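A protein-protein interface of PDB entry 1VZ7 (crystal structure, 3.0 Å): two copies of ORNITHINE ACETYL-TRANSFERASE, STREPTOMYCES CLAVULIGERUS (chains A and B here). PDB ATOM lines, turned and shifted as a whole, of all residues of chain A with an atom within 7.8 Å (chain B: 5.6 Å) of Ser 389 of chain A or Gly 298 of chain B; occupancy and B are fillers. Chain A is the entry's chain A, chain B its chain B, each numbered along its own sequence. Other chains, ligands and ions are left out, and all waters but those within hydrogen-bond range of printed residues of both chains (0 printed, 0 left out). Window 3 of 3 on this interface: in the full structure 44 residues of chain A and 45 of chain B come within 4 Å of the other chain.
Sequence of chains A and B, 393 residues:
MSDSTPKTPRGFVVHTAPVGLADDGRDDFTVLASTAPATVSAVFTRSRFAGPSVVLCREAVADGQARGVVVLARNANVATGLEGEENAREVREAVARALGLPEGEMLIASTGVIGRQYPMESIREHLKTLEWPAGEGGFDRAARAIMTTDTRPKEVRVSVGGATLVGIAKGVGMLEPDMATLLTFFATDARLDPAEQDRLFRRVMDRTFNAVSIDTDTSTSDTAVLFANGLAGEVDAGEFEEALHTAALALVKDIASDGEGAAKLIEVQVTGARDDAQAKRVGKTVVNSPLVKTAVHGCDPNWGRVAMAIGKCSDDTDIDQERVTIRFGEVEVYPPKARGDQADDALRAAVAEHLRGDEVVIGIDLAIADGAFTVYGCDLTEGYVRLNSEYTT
Gly 383 of chain A touches none of the printed residues of chain B. Ser 389 of chain A touches just these residues of chain B: Thr 294, His 297 and Gly 298. Of the printed residues of chain A, Thr 294 of chain B touches Asn 388 and Ser 389. Printed residues of chain A within 4 Å of Ala 295 of chain B: Asn 388. Of the printed residues of chain A, His 297 of chain B touches Ser 389. Of chain A, only Ser 389 comes within 4 Å of Gly 298 of chain B. Cys 299 of chain B touches none of the printed residues of chain A. Of the printed residues of chain A, Arg 305 of chain B touches Asn 388. The nearest printed residue of chain B that does not touch Val 385 of chain A is His 297 of chain B (4.1 Å).
The backbone carbonyl oxygen (O) of Asn 388 of chain A lies within hydrogen-bond range of the guanidinium group (NH1) of Arg 305 of chain B (3.0 Å).
The side-chain hydroxyl (OG1) of Thr 294 of chain B sits at hydrogen-bond distance from the guanidinium group (NH1) of Arg 305 of chain B. The side-chain carboxylate of Glu 260 of chain A sits close to the side-chain amide oxygen of Asn 388 of chain A. The backbone carbonyl oxygen of Ala 295 of chain B lies within hydrogen-bond range of the backbone NH of Asp 300 of chain B (3.1 Å). NE2 of His 297 of chain B sits at hydrogen-bond distance from OE2 of Glu 382 of chain B (2.9 Å). ND2 of Asn 388 of chain A lies within hydrogen-bond range of O of Tyr 384 of chain A, 2.9 Å away.
No position is printed for both chains.
Among the printed residues, merely in contact across the chains: Val 385 of chain A with Glu 382 of chain B, Asn 388 of chain A with Thr 294 of chain B, Asn 388 of chain A with Ala 295 of chain B, Ser 389 of chain A with Thr 294 of chain B, Ser 389 of chain A with His 297 of chain B and Ser 389 of chain A with Gly 298 of chain B.
Hydrophobic or aromatic side chains of chain A that line the printed part of chain B: Val 385. Of the 9 printed residues of chain B, 6 touch a printed residue of chain A. Hydrophobic or aromatic side chains of chain B within 4 Å of the printed part of chain A: His 297. Among the printed residues, 7 pairs touch across the chains. Among the printed residues, no Asp or Glu carboxylate lies within 4 Å of a Lys or Arg side-chain nitrogen of the other chain.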
ATOM      1  N   GLU A 260      29.414  -3.456  14.873  1.00  0.00           N
ATOM      2  CA  GLU A 260      28.751  -4.494  14.087  1.00  0.00           C
ATOM      3  C   GLU A 260      27.372  -4.905  14.592  1.00  0.00           C
ATOM      4  O   GLU A 260      27.240  -5.482  15.668  1.00  0.00           O
ATOM      5  CB  GLU A 260      29.634  -5.739  13.993  1.00  0.00           C
ATOM      6  CG  GLU A 260      30.977  -5.482  13.347  1.00  0.00           C
ATOM      7  CD  GLU A 260      31.607  -6.738  12.792  1.00  0.00           C
ATOM      8  OE1 GLU A 260      31.021  -7.320  11.852  1.00  0.00           O
ATOM      9  OE2 GLU A 260      32.684  -7.139  13.287  1.00  0.00           O
ATOM     10  N   GLY A 383      22.352  -9.436  14.761  1.00  0.00           N
ATOM     11  CA  GLY A 383      22.947  -9.006  13.508  1.00  0.00           C
ATOM     12  C   GLY A 383      24.449  -9.174  13.484  1.00  0.00           C
ATOM     13  O   GLY A 383      25.030  -9.337  12.416  1.00  0.00           O
ATOM     14  N   TYR A 384      25.080  -9.112  14.654  1.00  0.00           N
ATOM     15  CA  TYR A 384      26.524  -9.287  14.728  1.00  0.00           C
ATOM     16  C   TYR A 384      26.771 -10.743  14.415  1.00  0.00           C
ATOM     17  O   TYR A 384      27.743 -11.089  13.748  1.00  0.00           O
ATOM     18  CB  TYR A 384      27.058  -8.945  16.128  1.00  0.00           C
ATOM     19  CG  TYR A 384      28.508  -9.354  16.378  1.00  0.00           C
ATOM     20  CD1 TYR A 384      28.831 -10.653  16.803  1.00  0.00           C
ATOM     21  CD2 TYR A 384      29.553  -8.442  16.205  1.00  0.00           C
ATOM     22  CE1 TYR A 384      30.158 -11.030  17.056  1.00  0.00           C
ATOM     23  CE2 TYR A 384      30.887  -8.803  16.450  1.00  0.00           C
ATOM     24  CZ  TYR A 384      31.185 -10.100  16.881  1.00  0.00           C
ATOM     25  OH  TYR A 384      32.497 -10.441  17.162  1.00  0.00           O
ATOM     26  N   VAL A 385      25.868 -11.594  14.889  1.00  0.00           N
ATOM     27  CA  VAL A 385      26.000 -13.016  14.649  1.00  0.00           C
ATOM     28  C   VAL A 385      25.877 -13.250  13.163  1.00  0.00           C
ATOM     29  O   VAL A 385      26.794 -13.762  12.536  1.00  0.00           O
ATOM     30  CB  VAL A 385      24.922 -13.816  15.393  1.00  0.00           C
ATOM     31  CG1 VAL A 385      24.893 -15.242  14.878  1.00  0.00           C
ATOM     32  CG2 VAL A 385      25.217 -13.815  16.894  1.00  0.00           C
ATOM     33  N   ARG A 386      24.753 -12.845  12.593  1.00  0.00           N
ATOM     34  CA  ARG A 386      24.522 -13.022  11.164  1.00  0.00           C
ATOM     35  C   ARG A 386      25.713 -12.529  10.329  1.00  0.00           C
ATOM     36  O   ARG A 386      26.273 -13.274   9.527  1.00  0.00           O
ATOM     37  CB  ARG A 386      23.236 -12.297  10.759  1.00  0.00           C
ATOM     38  CG  ARG A 386      22.799 -12.556   9.345  1.00  0.00           C
ATOM     39  CD  ARG A 386      21.369 -12.089   9.094  1.00  0.00           C
ATOM     40  NE  ARG A 386      21.159 -10.673   9.400  1.00  0.00           N
ATOM     41  CZ  ARG A 386      20.642 -10.225  10.542  1.00  0.00           C
ATOM     42  NH1 ARG A 386      20.274 -11.085  11.485  1.00  0.00           N
ATOM     43  NH2 ARG A 386      20.505  -8.919  10.742  1.00  0.00           N
ATOM     44  N   LEU A 387      26.114 -11.281  10.539  1.00  0.00           N
ATOM     45  CA  LEU A 387      27.231 -10.699   9.798  1.00  0.00           C
ATOM     46  C   LEU A 387      28.552 -11.442   9.935  1.00  0.00           C
ATOM     47  O   LEU A 387      29.267 -11.629   8.953  1.00  0.00           O
ATOM     48  CB  LEU A 387      27.449  -9.248  10.227  1.00  0.00           C
ATOM     49  CG  LEU A 387      26.271  -8.310   9.994  1.00  0.00           C
ATOM     50  CD1 LEU A 387      26.621  -6.932  10.530  1.00  0.00           C
ATOM     51  CD2 LEU A 387      25.927  -8.266   8.505  1.00  0.00           C
ATOM     52  N   ASN A 388      28.887 -11.847  11.153  1.00  0.00           N
ATOM     53  CA  ASN A 388      30.147 -12.539  11.385  1.00  0.00           C
ATOM     54  C   ASN A 388      30.041 -14.039  11.236  1.00  0.00           C
ATOM     55  O   ASN A 388      31.022 -14.745  11.445  1.00  0.00           O
ATOM     56  CB  ASN A 388      30.687 -12.214  12.773  1.00  0.00           C
ATOM     57  CG  ASN A 388      31.100 -10.771  12.916  1.00  0.00           C
ATOM     58  OD1 ASN A 388      32.039 -10.313  12.267  1.00  0.00           O
ATOM     59  ND2 ASN A 388      30.401 -10.041  13.765  1.00  0.00           N
ATOM     60  N   SER A 389      28.856 -14.532  10.887  1.00  0.00           N
ATOM     61  CA  SER A 389      28.670 -15.966  10.699  1.00  0.00           C
ATOM     62  C   SER A 389      28.684 -16.281   9.211  1.00  0.00           C
ATOM     63  O   SER A 389      28.477 -17.424   8.812  1.00  0.00           O
ATOM     64  CB  SER A 389      27.347 -16.440  11.315  1.00  0.00           C
ATOM     65  N   GLU A 390      28.936 -15.269   8.389  1.00  0.00           N
ATOM     66  CA  GLU A 390      28.967 -15.464   6.947  1.00  0.00           C
ATOM     67  C   GLU A 390      30.307 -16.037   6.480  1.00  0.00           C
ATOM     68  O   GLU A 390      30.436 -17.245   6.251  1.00  0.00           O
ATOM     69  CB  GLU A 390      28.682 -14.137   6.237  1.00  0.00           C
ATOM     70  N   THR B 294      31.578 -17.399  16.369  1.00  0.00           N
ATOM     71  CA  THR B 294      30.639 -17.111  15.284  1.00  0.00           C
ATOM     72  C   THR B 294      31.002 -17.834  14.000  1.00  0.00           C
ATOM     73  O   THR B 294      30.137 -18.395  13.344  1.00  0.00           O
ATOM     74  CB  THR B 294      30.553 -15.597  14.994  1.00  0.00           C
ATOM     75  OG1 THR B 294      31.870 -15.030  14.953  1.00  0.00           O
ATOM     76  CG2 THR B 294      29.741 -14.914  16.064  1.00  0.00           C
ATOM     77  N   ALA B 295      32.276 -17.817  13.633  1.00  0.00           N
ATOM     78  CA  ALA B 295      32.719 -18.515  12.431  1.00  0.00           C
ATOM     79  C   ALA B 295      32.292 -19.973  12.585  1.00  0.00           C
ATOM     80  O   ALA B 295      31.592 -20.536  11.741  1.00  0.00           O
ATOM     81  CB  ALA B 295      34.234 -18.427  12.300  1.00  0.00           C
ATOM     82  N   VAL B 296      32.719 -20.576  13.686  1.00  0.00           N
ATOM     83  CA  VAL B 296      32.365 -21.945  13.978  1.00  0.00           C
ATOM     84  C   VAL B 296      30.878 -22.180  13.768  1.00  0.00           C
ATOM     85  O   VAL B 296      30.473 -23.250  13.313  1.00  0.00           O
ATOM     86  CB  VAL B 296      32.716 -22.283  15.419  1.00  0.00           C
ATOM     87  CG1 VAL B 296      32.214 -23.694  15.770  1.00  0.00           C
ATOM     88  CG2 VAL B 296      34.229 -22.148  15.605  1.00  0.00           C
ATOM     89  N   HIS B 297      30.066 -21.180  14.103  1.00  0.00           N
ATOM     90  CA  HIS B 297      28.623 -21.310  13.951  1.00  0.00           C
ATOM     91  C   HIS B 297      28.227 -21.276  12.485  1.00  0.00           C
ATOM     92  O   HIS B 297      27.211 -21.858  12.082  1.00  0.00           O
ATOM     93  CB  HIS B 297      27.889 -20.195  14.692  1.00  0.00           C
ATOM     94  CG  HIS B 297      26.439 -20.096  14.327  1.00  0.00           C
ATOM     95  ND1 HIS B 297      25.550 -21.134  14.524  1.00  0.00           N
ATOM     96  CD2 HIS B 297      25.743 -19.120  13.696  1.00  0.00           C
ATOM     97  CE1 HIS B 297      24.372 -20.805  14.022  1.00  0.00           C
ATOM     98  NE2 HIS B 297      24.463 -19.589  13.513  1.00  0.00           N
ATOM     99  N   GLY B 298      29.038 -20.588  11.691  1.00  0.00           N
ATOM    100  CA  GLY B 298      28.751 -20.470  10.276  1.00  0.00           C
ATOM    101  C   GLY B 298      29.374 -21.570   9.441  1.00  0.00           C
ATOM    102  O   GLY B 298      29.288 -21.537   8.216  1.00  0.00           O
ATOM    103  N   CYS B 299      29.981 -22.551  10.102  1.00  0.00           N
ATOM    104  CA  CYS B 299      30.636 -23.648   9.401  1.00  0.00           C
ATOM    105  C   CYS B 299      31.846 -23.090   8.637  1.00  0.00           C
ATOM    106  O   CYS B 299      32.126 -23.486   7.506  1.00  0.00           O
ATOM    107  CB  CYS B 299      29.653 -24.327   8.441  1.00  0.00           C
ATOM    108  SG  CYS B 299      28.293 -25.198   9.266  1.00  0.00           S
ATOM    109  N   ASP B 300      32.557 -22.168   9.284  1.00  0.00           N
ATOM    110  CA  ASP B 300      33.724 -21.516   8.705  1.00  0.00           C
ATOM    111  C   ASP B 300      34.992 -21.889   9.454  1.00  0.00           C
ATOM    112  O   ASP B 300      35.129 -21.583  10.634  1.00  0.00           O
ATOM    113  CB  ASP B 300      33.546 -19.994   8.753  1.00  0.00           C
ATOM    114  CG  ASP B 300      34.671 -19.246   8.048  1.00  0.00           C
ATOM    115  OD1 ASP B 300      35.797 -19.201   8.576  1.00  0.00           O
ATOM    116  OD2 ASP B 300      34.429 -18.700   6.950  1.00  0.00           O
ATOM    117  N   ARG B 305      40.858 -16.068  12.626  1.00  0.00           N
ATOM    118  CA  ARG B 305      40.238 -15.583  13.850  1.00  0.00           C
ATOM    119  C   ARG B 305      40.797 -16.354  15.038  1.00  0.00           C
ATOM    120  O   ARG B 305      40.982 -15.777  16.109  1.00  0.00           O
ATOM    121  CB  ARG B 305      38.717 -15.742  13.793  1.00  0.00           C
ATOM    122  CG  ARG B 305      38.027 -14.787  12.829  1.00  0.00           C
ATOM    123  CD  ARG B 305      36.525 -14.933  12.884  1.00  0.00           C
ATOM    124  NE  ARG B 305      35.860 -13.994  11.988  1.00  0.00           N
ATOM    125  CZ  ARG B 305      34.543 -13.790  11.939  1.00  0.00           C
ATOM    126  NH1 ARG B 305      33.722 -14.459  12.735  1.00  0.00           N
ATOM    127  NH2 ARG B 305      34.042 -12.904  11.094  1.00  0.00           N
ATOM    128  N   GLU B 382      22.144 -17.265  16.763  1.00  0.00           N
ATOM    129  CA  GLU B 382      21.214 -16.146  16.880  1.00  0.00           C
ATOM    130  C   GLU B 382      20.160 -16.450  17.949  1.00  0.00           C
ATOM    131  O   GLU B 382      19.333 -15.599  18.273  1.00  0.00           O
ATOM    132  CB  GLU B 382      20.525 -15.875  15.535  1.00  0.00           C
ATOM    133  CG  GLU B 382      21.463 -15.593  14.357  1.00  0.00           C
ATOM    134  CD  GLU B 382      21.707 -16.816  13.475  1.00  0.00           C
ATOM    135  OE1 GLU B 382      20.718 -17.406  12.977  1.00  0.00           O
ATOM    136  OE2 GLU B 382      22.887 -17.180  13.273  1.00  0.00           O
